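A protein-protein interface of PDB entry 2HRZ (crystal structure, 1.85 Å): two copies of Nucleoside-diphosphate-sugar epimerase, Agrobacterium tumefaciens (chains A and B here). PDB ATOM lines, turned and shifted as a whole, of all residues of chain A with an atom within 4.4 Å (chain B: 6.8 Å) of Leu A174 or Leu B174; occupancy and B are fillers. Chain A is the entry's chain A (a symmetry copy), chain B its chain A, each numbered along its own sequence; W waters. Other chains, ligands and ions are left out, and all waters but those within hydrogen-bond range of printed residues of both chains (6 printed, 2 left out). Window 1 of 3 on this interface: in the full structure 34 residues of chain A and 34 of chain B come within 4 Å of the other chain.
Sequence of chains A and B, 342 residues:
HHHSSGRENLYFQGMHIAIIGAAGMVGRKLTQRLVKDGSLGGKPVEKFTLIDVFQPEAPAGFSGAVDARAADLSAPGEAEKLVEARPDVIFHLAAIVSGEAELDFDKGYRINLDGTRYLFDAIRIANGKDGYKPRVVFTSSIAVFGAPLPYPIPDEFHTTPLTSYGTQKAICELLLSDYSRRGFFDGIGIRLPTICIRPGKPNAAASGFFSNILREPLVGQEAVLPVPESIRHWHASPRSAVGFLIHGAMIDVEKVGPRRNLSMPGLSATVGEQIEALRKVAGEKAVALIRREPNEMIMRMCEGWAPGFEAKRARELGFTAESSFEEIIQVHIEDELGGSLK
Water W2 lies within hydrogen-bond range of the side-chain hydroxyl (OG1) of Thr A159 (2.6 Å) and the side-chain hydroxyl (OG1) of Thr B159 (3.1 Å). Water W6 bridges OG1 of Thr B159 and OG1 of Thr A159. Water W3 bridges the backbone carbonyl oxygen (O) of Leu A174 (2.7 Å) and the side-chain hydroxyl (OG1) of Thr B167 (2.9 Å). Water W4 bridges O of Leu B174 (2.7 Å) and OG1 of Thr A167 (2.9 Å). Water W5 lies within hydrogen-bond range of OD1 of Asp A178 (2.8 Å) and O of Pro B161 (2.8 Å). Water W1 lies within hydrogen-bond range of the side-chain carboxylate (OD1) of Asp B178 (2.8 Å) and the backbone carbonyl oxygen (O) of Pro A161 (2.8 Å).
Among the printed residues, merely in contact across the chains: Thr A159 with Leu B174 (3.6 Å), Pro A161 with Leu B174 (3.8 Å), Thr A167 with Leu B174 (3.7 Å), Ala A170 with Leu B174 (3.6 Å), Ile A171 with Ile B171 (3.6 Å), Ile A171 with Leu B174 (3.8 Å), Ile A171 with Leu B175 (3.7 Å), Leu A174 with Thr B159 (3.6 Å), Leu A174 with Pro B161 (3.8 Å), Leu A174 with Thr B167 (3.7 Å), Leu A174 with Ala B170 (3.6 Å), Leu A174 with Ile B171 (3.8 Å), Leu A174 with Leu B174 (3.6 Å), Leu A175 with Tyr B109 (3.7 Å) and Leu A175 with Ile B171 (3.7 Å).
Thr A167 touches Asp B178, and with the chains exchanged Asp A178 touches Thr B167. Ala A170 touches Leu B174, and with the chains exchanged Leu A174 touches Ala B170. Ile A171 touches its own counterpart, Ile B171. Leu B174 touches its own counterpart, Leu A174. Positions printed for both chains: 159, 161, 167, 170, 171, 172, 173, 174, 175, 176, 177 and 178. Of the 18 pairs that touch across the chains among the printed residues, 16 have their exchanged pair printed and touching as well.
Of the 21 printed residues of chain B, 9 touch a printed residue of chain A. Hydrophobic or aromatic side chains of chain B within 4 Å of the printed part of chain A: Tyr B109, Pro B161, Ala B170, Ile B171, Leu B174 and Leu B175. Along chain B the printed residues that touch a printed residue of chain A span positions 109 to 178. Hydrophobic or aromatic side chains of chain A that line the printed part of chain B: Pro A161, Ala A170, Ile A171, Leu A174 and Leu A175. Along chain A the printed residues that touch a printed residue of chain B span positions 159 to 178. Among the printed residues, 18 pairs touch across the chains. Among the printed residues, no Asp or Glu carboxylate lies within 4 Å of a Lys or Arg side-chain nitrogen of the other chain.
The backbone NH of Tyr B109 sits close to the side-chain amide oxygen of Gln B168 (3.3 Å).
The side-chain carboxylate (OD2) of Asp A178 lies within hydrogen-bond range of the side-chain hydroxyl (OH) of Tyr B109, 2.6 Å away. The side-chain carboxylate of Asp A178 sits at hydrogen-bond distance from the side-chain hydroxyl of Thr B167 (3.4 Å). The side-chain hydroxyl (OG1) of Thr A167 sits at hydrogen-bond distance from the side-chain carboxylate (OD1) of Asp B178.
Printed residues of chain B within 4 Å of Thr A159: Leu B174 (3.6 Å). Of chain B, only Thr B159 (3.6 Å), Pro B161 (3.8 Å), Thr B167 (3.7 Å), Ala B170 (3.6 Å), Ile B171 (3.8 Å) and Leu B174 (3.6 Å) come within 4 Å of Leu A174. Gln B168 touches none of the printed residues of chain A. Of chain A, only Thr A159 (3.6 Å), Pro A161 (3.8 Å), Thr A167 (3.7 Å), Ala A170 (3.6 Å), Ile A171 (3.8 Å) and Leu A174 (3.6 Å) come within 4 Å of Leu B174. Of the printed residues of chain A, Leu B175 touches Ile A171 (3.7 Å). The nearest printed residue of chain A that does not touch Thr B167 is Leu A175 (4.5 Å).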
ATOM      1  N   THR A 159     -21.204  20.396  27.648  1.00  0.00           N
ATOM      2  CA  THR A 159     -19.945  19.791  27.230  1.00  0.00           C
ATOM      3  C   THR A 159     -19.145  20.794  26.416  1.00  0.00           C
ATOM      4  O   THR A 159     -19.503  21.093  25.271  1.00  0.00           O
ATOM      5  CB  THR A 159     -20.180  18.494  26.389  1.00  0.00           C
ATOM      6  OG1 THR A 159     -20.985  18.802  25.236  1.00  0.00           O
ATOM      7  CG2 THR A 159     -20.880  17.405  27.254  1.00  0.00           C
ATOM      8  N   PRO A 161     -15.438  20.678  25.749  1.00  0.00           N
ATOM      9  CA  PRO A 161     -14.126  20.052  25.895  1.00  0.00           C
ATOM     10  C   PRO A 161     -13.009  20.903  25.320  1.00  0.00           C
ATOM     11  O   PRO A 161     -13.190  21.566  24.291  1.00  0.00           O
ATOM     12  CB  PRO A 161     -14.270  18.722  25.128  1.00  0.00           C
ATOM     13  CG  PRO A 161     -15.373  18.943  24.154  1.00  0.00           C
ATOM     14  CD  PRO A 161     -16.305  19.945  24.809  1.00  0.00           C
ATOM     15  N   THR A 167     -13.764  16.473  22.345  1.00  0.00           N
ATOM     16  CA  THR A 167     -14.633  16.947  21.273  1.00  0.00           C
ATOM     17  C   THR A 167     -15.236  15.745  20.529  1.00  0.00           C
ATOM     18  O   THR A 167     -16.456  15.683  20.310  1.00  0.00           O
ATOM     19  CB  THR A 167     -13.863  17.868  20.287  1.00  0.00           C
ATOM     20  OG1 THR A 167     -13.414  19.041  20.989  1.00  0.00           O
ATOM     21  CG2 THR A 167     -14.780  18.267  19.104  1.00  0.00           C
ATOM     22  N   ALA A 170     -17.827  13.983  22.674  1.00  0.00           N
ATOM     23  CA  ALA A 170     -19.047  14.804  22.798  1.00  0.00           C
ATOM     24  C   ALA A 170     -19.884  14.714  21.512  1.00  0.00           C
ATOM     25  O   ALA A 170     -21.103  14.681  21.557  1.00  0.00           O
ATOM     26  CB  ALA A 170     -18.694  16.280  23.130  1.00  0.00           C
ATOM     27  N   ILE A 171     -19.221  14.687  20.365  1.00  0.00           N
ATOM     28  CA  ILE A 171     -19.942  14.547  19.102  1.00  0.00           C
ATOM     29  C   ILE A 171     -20.555  13.138  18.987  1.00  0.00           C
ATOM     30  O   ILE A 171     -21.699  12.983  18.569  1.00  0.00           O
ATOM     31  CB  ILE A 171     -19.027  14.866  17.902  1.00  0.00           C
ATOM     32  CG1 ILE A 171     -18.676  16.367  17.880  1.00  0.00           C
ATOM     33  CG2 ILE A 171     -19.670  14.371  16.576  1.00  0.00           C
ATOM     34  CD1 ILE A 171     -17.500  16.680  16.976  1.00  0.00           C
ATOM     35  N   CYS A 172     -19.795  12.111  19.347  1.00  0.00           N
ATOM     36  CA  CYS A 172     -20.317  10.730  19.325  1.00  0.00           C
ATOM     37  C   CYS A 172     -21.548  10.604  20.233  1.00  0.00           C
ATOM     38  O   CYS A 172     -22.539   9.971  19.869  1.00  0.00           O
ATOM     39  CB  CYS A 172     -19.230   9.747  19.768  1.00  0.00           C
ATOM     40  SG  CYS A 172     -17.921   9.500  18.534  1.00  0.00           S
ATOM     41  N   GLU A 173     -21.491  11.226  21.409  1.00  0.00           N
ATOM     42  CA  GLU A 173     -22.664  11.272  22.304  1.00  0.00           C
ATOM     43  C   GLU A 173     -23.925  11.801  21.606  1.00  0.00           C
ATOM     44  O   GLU A 173     -25.009  11.219  21.734  1.00  0.00           O
ATOM     45  CB  GLU A 173     -22.369  12.165  23.511  1.00  0.00           C
ATOM     46  CG  GLU A 173     -21.357  11.595  24.518  1.00  0.00           C
ATOM     47  CD  GLU A 173     -21.323  12.385  25.827  1.00  0.00           C
ATOM     48  OE1 GLU A 173     -21.990  13.442  25.928  1.00  0.00           O
ATOM     49  OE2 GLU A 173     -20.643  11.935  26.761  1.00  0.00           O
ATOM     50  N   LEU A 174     -23.787  12.929  20.906  1.00  0.00           N
ATOM     51  CA  LEU A 174     -24.909  13.563  20.188  1.00  0.00           C
ATOM     52  C   LEU A 174     -25.450  12.648  19.084  1.00  0.00           C
ATOM     53  O   LEU A 174     -26.677  12.494  18.941  1.00  0.00           O
ATOM     54  CB  LEU A 174     -24.491  14.929  19.615  1.00  0.00           C
ATOM     55  CG  LEU A 174     -24.334  16.056  20.652  1.00  0.00           C
ATOM     56  CD1 LEU A 174     -23.511  17.195  20.117  1.00  0.00           C
ATOM     57  CD2 LEU A 174     -25.709  16.592  21.121  1.00  0.00           C
ATOM     58  N   LEU A 175     -24.547  12.034  18.323  1.00  0.00           N
ATOM     59  CA  LEU A 175     -24.959  11.079  17.292  1.00  0.00           C
ATOM     60  C   LEU A 175     -25.700   9.897  17.931  1.00  0.00           C
ATOM     61  O   LEU A 175     -26.746   9.463  17.442  1.00  0.00           O
ATOM     62  CB  LEU A 175     -23.746  10.564  16.504  1.00  0.00           C
ATOM     63  CG  LEU A 175     -23.071  11.596  15.581  1.00  0.00           C
ATOM     64  CD1 LEU A 175     -21.728  11.034  15.071  1.00  0.00           C
ATOM     65  CD2 LEU A 175     -23.990  11.960  14.412  1.00  0.00           C
ATOM     66  N   LEU A 176     -25.148   9.391  19.024  1.00  0.00           N
ATOM     67  CA  LEU A 176     -25.769   8.273  19.754  1.00  0.00           C
ATOM     68  C   LEU A 176     -27.206   8.613  20.176  1.00  0.00           C
ATOM     69  O   LEU A 176     -28.110   7.816  19.943  1.00  0.00           O
ATOM     70  CB  LEU A 176     -24.898   7.857  20.948  1.00  0.00           C
ATOM     71  CG  LEU A 176     -25.429   6.659  21.768  1.00  0.00           C
ATOM     72  CD1 LEU A 176     -24.277   5.891  22.416  1.00  0.00           C
ATOM     73  CD2 LEU A 176     -26.422   7.122  22.845  1.00  0.00           C
ATOM     74  N   SER A 177     -27.427   9.790  20.768  1.00  0.00           N
ATOM     75  CA  SER A 177     -28.793  10.160  21.170  1.00  0.00           C
ATOM     76  C   SER A 177     -29.737  10.295  19.969  1.00  0.00           C
ATOM     77  O   SER A 177     -30.908   9.899  20.056  1.00  0.00           O
ATOM     78  CB  SER A 177     -28.822  11.431  22.016  1.00  0.00           C
ATOM     79  OG  SER A 177     -28.224  11.217  23.282  1.00  0.00           O
ATOM     80  N   ASP A 178     -29.257  10.887  18.869  1.00  0.00           N
ATOM     81  CA  ASP A 178     -30.126  11.108  17.697  1.00  0.00           C
ATOM     82  C   ASP A 178     -30.498   9.803  16.983  1.00  0.00           C
ATOM     83  O   ASP A 178     -31.663   9.593  16.622  1.00  0.00           O
ATOM     84  CB  ASP A 178     -29.509  12.102  16.701  1.00  0.00           C
ATOM     85  CG  ASP A 178     -30.536  12.670  15.741  1.00  0.00           C
ATOM     86  OD1 ASP A 178     -31.601  13.139  16.204  1.00  0.00           O
ATOM     87  OD2 ASP A 178     -30.280  12.647  14.520  1.00  0.00           O
ATOM     88  N   TYR B 109     -28.125  15.309   7.365  1.00  0.00           N
ATOM     89  CA  TYR B 109     -26.743  15.082   7.798  1.00  0.00           C
ATOM     90  C   TYR B 109     -25.731  15.518   6.754  1.00  0.00           C
ATOM     91  O   TYR B 109     -24.688  16.053   7.098  1.00  0.00           O
ATOM     92  CB  TYR B 109     -26.498  13.639   8.235  1.00  0.00           C
ATOM     93  CG  TYR B 109     -26.868  13.452   9.690  1.00  0.00           C
ATOM     94  CD1 TYR B 109     -28.132  12.996  10.058  1.00  0.00           C
ATOM     95  CD2 TYR B 109     -25.963  13.796  10.695  1.00  0.00           C
ATOM     96  CE1 TYR B 109     -28.490  12.866  11.435  1.00  0.00           C
ATOM     97  CE2 TYR B 109     -26.285  13.660  12.035  1.00  0.00           C
ATOM     98  CZ  TYR B 109     -27.546  13.212  12.406  1.00  0.00           C
ATOM     99  OH  TYR B 109     -27.817  13.093  13.746  1.00  0.00           O
ATOM    100  N   PHE B 120     -14.836  23.322   7.262  1.00  0.00           N
ATOM    101  CA  PHE B 120     -13.889  23.461   8.364  1.00  0.00           C
ATOM    102  C   PHE B 120     -12.557  22.781   8.033  1.00  0.00           C
ATOM    103  O   PHE B 120     -11.485  23.345   8.291  1.00  0.00           O
ATOM    104  CB  PHE B 120     -14.486  22.887   9.652  1.00  0.00           C
ATOM    105  CG  PHE B 120     -15.570  23.746  10.279  1.00  0.00           C
ATOM    106  CD1 PHE B 120     -16.025  24.919   9.666  1.00  0.00           C
ATOM    107  CD2 PHE B 120     -16.161  23.347  11.479  1.00  0.00           C
ATOM    108  CE1 PHE B 120     -17.013  25.706  10.255  1.00  0.00           C
ATOM    109  CE2 PHE B 120     -17.170  24.108  12.076  1.00  0.00           C
ATOM    110  CZ  PHE B 120     -17.609  25.281  11.473  1.00  0.00           C
ATOM    111  N   VAL B 144     -30.573  23.479  19.405  1.00  0.00           N
ATOM    112  CA  VAL B 144     -29.596  22.608  20.083  1.00  0.00           C
ATOM    113  C   VAL B 144     -30.084  22.182  21.461  1.00  0.00           C
ATOM    114  O   VAL B 144     -29.545  21.241  22.070  1.00  0.00           O
ATOM    115  CB  VAL B 144     -28.152  23.217  20.187  1.00  0.00           C
ATOM    116  CG1 VAL B 144     -27.580  23.514  18.790  1.00  0.00           C
ATOM    117  CG2 VAL B 144     -28.073  24.451  21.098  1.00  0.00           C
ATOM    118  N   THR B 159     -26.606  20.749  25.733  1.00  0.00           N
ATOM    119  CA  THR B 159     -27.315  20.621  24.466  1.00  0.00           C
ATOM    120  C   THR B 159     -27.794  19.189  24.295  1.00  0.00           C
ATOM    121  O   THR B 159     -26.983  18.286  24.053  1.00  0.00           O
ATOM    122  CB  THR B 159     -26.411  21.026  23.256  1.00  0.00           C
ATOM    123  OG1 THR B 159     -25.226  20.210  23.241  1.00  0.00           O
ATOM    124  CG2 THR B 159     -26.023  22.531  23.347  1.00  0.00           C
ATOM    125  N   THR B 160     -29.102  18.974  24.458  1.00  0.00           N
ATOM    126  CA  THR B 160     -29.718  17.656  24.263  1.00  0.00           C
ATOM    127  C   THR B 160     -30.869  17.748  23.261  1.00  0.00           C
ATOM    128  O   THR B 160     -32.054  17.584  23.625  1.00  0.00           O
ATOM    129  CB  THR B 160     -30.193  17.019  25.594  1.00  0.00           C
ATOM    130  OG1 THR B 160     -31.184  17.851  26.215  1.00  0.00           O
ATOM    131  CG2 THR B 160     -29.017  16.814  26.560  1.00  0.00           C
ATOM    132  N   PRO B 161     -30.531  18.012  21.987  1.00  0.00           N
ATOM    133  CA  PRO B 161     -31.564  18.266  20.985  1.00  0.00           C
ATOM    134  C   PRO B 161     -32.395  17.033  20.682  1.00  0.00           C
ATOM    135  O   PRO B 161     -31.870  15.912  20.659  1.00  0.00           O
ATOM    136  CB  PRO B 161     -30.766  18.723  19.748  1.00  0.00           C
ATOM    137  CG  PRO B 161     -29.403  18.155  19.922  1.00  0.00           C
ATOM    138  CD  PRO B 161     -29.173  18.089  21.420  1.00  0.00           C
ATOM    139  N   GLY B 166     -31.171  19.924  15.245  1.00  0.00           N
ATOM    140  CA  GLY B 166     -30.540  20.408  16.476  1.00  0.00           C
ATOM    141  C   GLY B 166     -29.267  19.629  16.775  1.00  0.00           C
ATOM    142  O   GLY B 166     -28.284  20.185  17.282  1.00  0.00           O
ATOM    143  N   THR B 167     -29.296  18.337  16.470  1.00  0.00           N
ATOM    144  CA  THR B 167     -28.134  17.471  16.643  1.00  0.00           C
ATOM    145  C   THR B 167     -26.992  17.955  15.735  1.00  0.00           C
ATOM    146  O   THR B 167     -25.849  18.119  16.187  1.00  0.00           O
ATOM    147  CB  THR B 167     -28.483  15.988  16.337  1.00  0.00           C
ATOM    148  OG1 THR B 167     -29.468  15.531  17.281  1.00  0.00           O
ATOM    149  CG2 THR B 167     -27.208  15.113  16.423  1.00  0.00           C
ATOM    150  N   GLN B 168     -27.306  18.168  14.463  1.00  0.00           N
ATOM    151  CA  GLN B 168     -26.329  18.655  13.486  1.00  0.00           C
ATOM    152  C   GLN B 168     -25.697  19.985  13.919  1.00  0.00           C
ATOM    153  O   GLN B 168     -24.472  20.140  13.874  1.00  0.00           O
ATOM    154  CB  GLN B 168     -26.985  18.768  12.095  1.00  0.00           C
ATOM    155  CG  GLN B 168     -27.270  17.359  11.480  1.00  0.00           C
ATOM    156  CD  GLN B 168     -28.596  17.234  10.724  1.00  0.00           C
ATOM    157  OE1 GLN B 168     -29.052  16.109  10.411  1.00  0.00           O
ATOM    158  NE2 GLN B 168     -29.228  18.356  10.453  1.00  0.00           N
ATOM    159  N   LYS B 169     -26.527  20.922  14.363  1.00  0.00           N
ATOM    160  CA  LYS B 169     -26.027  22.208  14.852  1.00  0.00           C
ATOM    161  C   LYS B 169     -25.109  22.052  16.077  1.00  0.00           C
ATOM    162  O   LYS B 169     -24.046  22.705  16.145  1.00  0.00           O
ATOM    163  CB  LYS B 169     -27.186  23.180  15.161  1.00  0.00           C
ATOM    164  CG  LYS B 169     -27.953  23.675  13.909  1.00  0.00           C
ATOM    165  CD  LYS B 169     -27.026  24.307  12.853  1.00  0.00           C
ATOM    166  CE  LYS B 169     -27.806  25.183  11.873  1.00  0.00           C
ATOM    167  NZ  LYS B 169     -26.861  25.790  10.890  1.00  0.00           N
ATOM    168  N   ALA B 170     -25.520  21.209  17.023  1.00  0.00           N
ATOM    169  CA  ALA B 170     -24.742  20.978  18.256  1.00  0.00           C
ATOM    170  C   ALA B 170     -23.376  20.362  17.916  1.00  0.00           C
ATOM    171  O   ALA B 170     -22.373  20.684  18.533  1.00  0.00           O
ATOM    172  CB  ALA B 170     -25.528  20.080  19.250  1.00  0.00           C
ATOM    173  N   ILE B 171     -23.347  19.466  16.941  1.00  0.00           N
ATOM    174  CA  ILE B 171     -22.078  18.876  16.523  1.00  0.00           C
ATOM    175  C   ILE B 171     -21.199  19.929  15.823  1.00  0.00           C
ATOM    176  O   ILE B 171     -19.998  20.010  16.068  1.00  0.00           O
ATOM    177  CB  ILE B 171     -22.308  17.643  15.624  1.00  0.00           C
ATOM    178  CG1 ILE B 171     -22.920  16.489  16.444  1.00  0.00           C
ATOM    179  CG2 ILE B 171     -20.995  17.244  14.895  1.00  0.00           C
ATOM    180  CD1 ILE B 171     -23.516  15.402  15.570  1.00  0.00           C
ATOM    181  N   CYS B 172     -21.790  20.731  14.946  1.00  0.00           N
ATOM    182  CA  CYS B 172     -21.040  21.809  14.270  1.00  0.00           C
ATOM    183  C   CYS B 172     -20.441  22.777  15.299  1.00  0.00           C
ATOM    184  O   CYS B 172     -19.292  23.198  15.175  1.00  0.00           O
ATOM    185  CB  CYS B 172     -21.957  22.564  13.303  1.00  0.00           C
ATOM    186  SG  CYS B 172     -22.376  21.625  11.808  1.00  0.00           S
ATOM    187  N   GLU B 173     -21.217  23.115  16.328  1.00  0.00           N
ATOM    188  CA  GLU B 173     -20.697  23.939  17.436  1.00  0.00           C
ATOM    189  C   GLU B 173     -19.408  23.373  18.046  1.00  0.00           C
ATOM    190  O   GLU B 173     -18.439  24.108  18.271  1.00  0.00           O
ATOM    191  CB  GLU B 173     -21.747  24.053  18.543  1.00  0.00           C
ATOM    192  CG  GLU B 173     -22.975  24.911  18.198  1.00  0.00           C
ATOM    193  CD  GLU B 173     -23.835  25.224  19.424  1.00  0.00           C
ATOM    194  OE1 GLU B 173     -23.560  24.689  20.525  1.00  0.00           O
ATOM    195  OE2 GLU B 173     -24.776  26.021  19.287  1.00  0.00           O
ATOM    196  N   LEU B 174     -19.418  22.074  18.353  1.00  0.00           N
ATOM    197  CA  LEU B 174     -18.257  21.388  18.953  1.00  0.00           C
ATOM    198  C   LEU B 174     -17.049  21.414  18.011  1.00  0.00           C
ATOM    199  O   LEU B 174     -15.918  21.695  18.447  1.00  0.00           O
ATOM    200  CB  LEU B 174     -18.617  19.945  19.349  1.00  0.00           C
ATOM    201  CG  LEU B 174     -19.517  19.809  20.591  1.00  0.00           C
ATOM    202  CD1 LEU B 174     -20.185  18.463  20.650  1.00  0.00           C
ATOM    203  CD2 LEU B 174     -18.722  20.046  21.897  1.00  0.00           C
ATOM    204  N   LEU B 175     -17.286  21.140  16.730  1.00  0.00           N
ATOM    205  CA  LEU B 175     -16.214  21.213  15.735  1.00  0.00           C
ATOM    206  C   LEU B 175     -15.658  22.642  15.663  1.00  0.00           C
ATOM    207  O   LEU B 175     -14.442  22.849  15.631  1.00  0.00           O
ATOM    208  CB  LEU B 175     -16.718  20.783  14.351  1.00  0.00           C
ATOM    209  CG  LEU B 175     -17.044  19.285  14.202  1.00  0.00           C
ATOM    210  CD1 LEU B 175     -17.787  19.046  12.871  1.00  0.00           C
ATOM    211  CD2 LEU B 175     -15.766  18.443  14.274  1.00  0.00           C
ATOM    212  N   LEU B 176     -16.559  23.613  15.640  1.00  0.00           N
ATOM    213  CA  LEU B 176     -16.162  25.031  15.598  1.00  0.00           C
ATOM    214  C   LEU B 176     -15.247  25.387  16.779  1.00  0.00           C
ATOM    215  O   LEU B 176     -14.201  25.994  16.573  1.00  0.00           O
ATOM    216  CB  LEU B 176     -17.400  25.936  15.530  1.00  0.00           C
ATOM    217  CG  LEU B 176     -17.107  27.451  15.439  1.00  0.00           C
ATOM    218  CD1 LEU B 176     -18.227  28.177  14.695  1.00  0.00           C
ATOM    219  CD2 LEU B 176     -16.920  28.063  16.835  1.00  0.00           C
ATOM    220  N   SER B 177     -15.619  24.999  18.003  1.00  0.00           N
ATOM    221  CA  SER B 177     -14.760  25.307  19.158  1.00  0.00           C
ATOM    222  C   SER B 177     -13.396  24.611  19.070  1.00  0.00           C
ATOM    223  O   SER B 177     -12.374  25.208  19.441  1.00  0.00           O
ATOM    224  CB  SER B 177     -15.439  24.982  20.485  1.00  0.00           C
ATOM    225  OG  SER B 177     -16.530  25.852  20.730  1.00  0.00           O
ATOM    226  N   ASP B 178     -13.373  23.349  18.628  1.00  0.00           N
ATOM    227  CA  ASP B 178     -12.105  22.596  18.577  1.00  0.00           C
ATOM    228  C   ASP B 178     -11.150  23.122  17.499  1.00  0.00           C
ATOM    229  O   ASP B 178      -9.948  23.283  17.748  1.00  0.00           O
ATOM    230  CB  ASP B 178     -12.337  21.088  18.391  1.00  0.00           C
ATOM    231  CG  ASP B 178     -11.120  20.266  18.768  1.00  0.00           C
ATOM    232  OD1 ASP B 178     -10.566  20.478  19.871  1.00  0.00           O
ATOM    233  OD2 ASP B 178     -10.714  19.407  17.960  1.00  0.00           O
ATOM    234  N   TYR B 179     -11.680  23.384  16.304  1.00  0.00           N
ATOM    235  CA  TYR B 179     -10.858  23.966  15.225  1.00  0.00           C
ATOM    236  C   TYR B 179     -10.346  25.358  15.578  1.00  0.00           C
ATOM    237  O   TYR B 179      -9.213  25.724  15.221  1.00  0.00           O
ATOM    238  CB  TYR B 179     -11.653  24.030  13.925  1.00  0.00           C
ATOM    239  CG  TYR B 179     -11.783  22.694  13.209  1.00  0.00           C
ATOM    240  CD1 TYR B 179     -12.321  21.561  13.859  1.00  0.00           C
ATOM    241  CD2 TYR B 179     -11.403  22.568  11.868  1.00  0.00           C
ATOM    242  CE1 TYR B 179     -12.457  20.320  13.175  1.00  0.00           C
ATOM    243  CE2 TYR B 179     -11.541  21.363  11.182  1.00  0.00           C
ATOM    244  CZ  TYR B 179     -12.065  20.239  11.840  1.00  0.00           C
ATOM    245  OH  TYR B 179     -12.193  19.049  11.140  1.00  0.00           O
ATOM    246  N   ASN B 261     -19.443  29.157  21.334  1.00  0.00           N
ATOM    247  CA  ASN B 261     -20.868  29.110  20.930  1.00  0.00           C
ATOM    248  C   ASN B 261     -21.733  29.798  21.961  1.00  0.00           C
ATOM    249  O   ASN B 261     -21.725  29.414  23.129  1.00  0.00           O
ATOM    250  CB  ASN B 261     -21.301  27.663  20.696  1.00  0.00           C
ATOM    251  CG  ASN B 261     -20.442  27.012  19.653  1.00  0.00           C
ATOM    252  OD1 ASN B 261     -20.555  27.341  18.474  1.00  0.00           O
ATOM    253  ND2 ASN B 261     -19.507  26.151  20.085  1.00  0.00           N
HETATM  254  O   HOH W   1     -11.680  21.929  21.963  1.00  0.00           O
HETATM  255  O   HOH W   2     -23.222  18.006  24.074  1.00  0.00           O
HETATM  256  O   HOH W   3     -28.441  14.417  19.737  1.00  0.00           O
HETATM  257  O   HOH W   4     -15.265  21.254  21.059  1.00  0.00           O
HETATM  258  O   HOH W   5     -32.040  13.760  18.877  1.00  0.00           O
HETATM  259  O   HOH W   6     -22.597  20.482  23.200  1.00  0.00           O
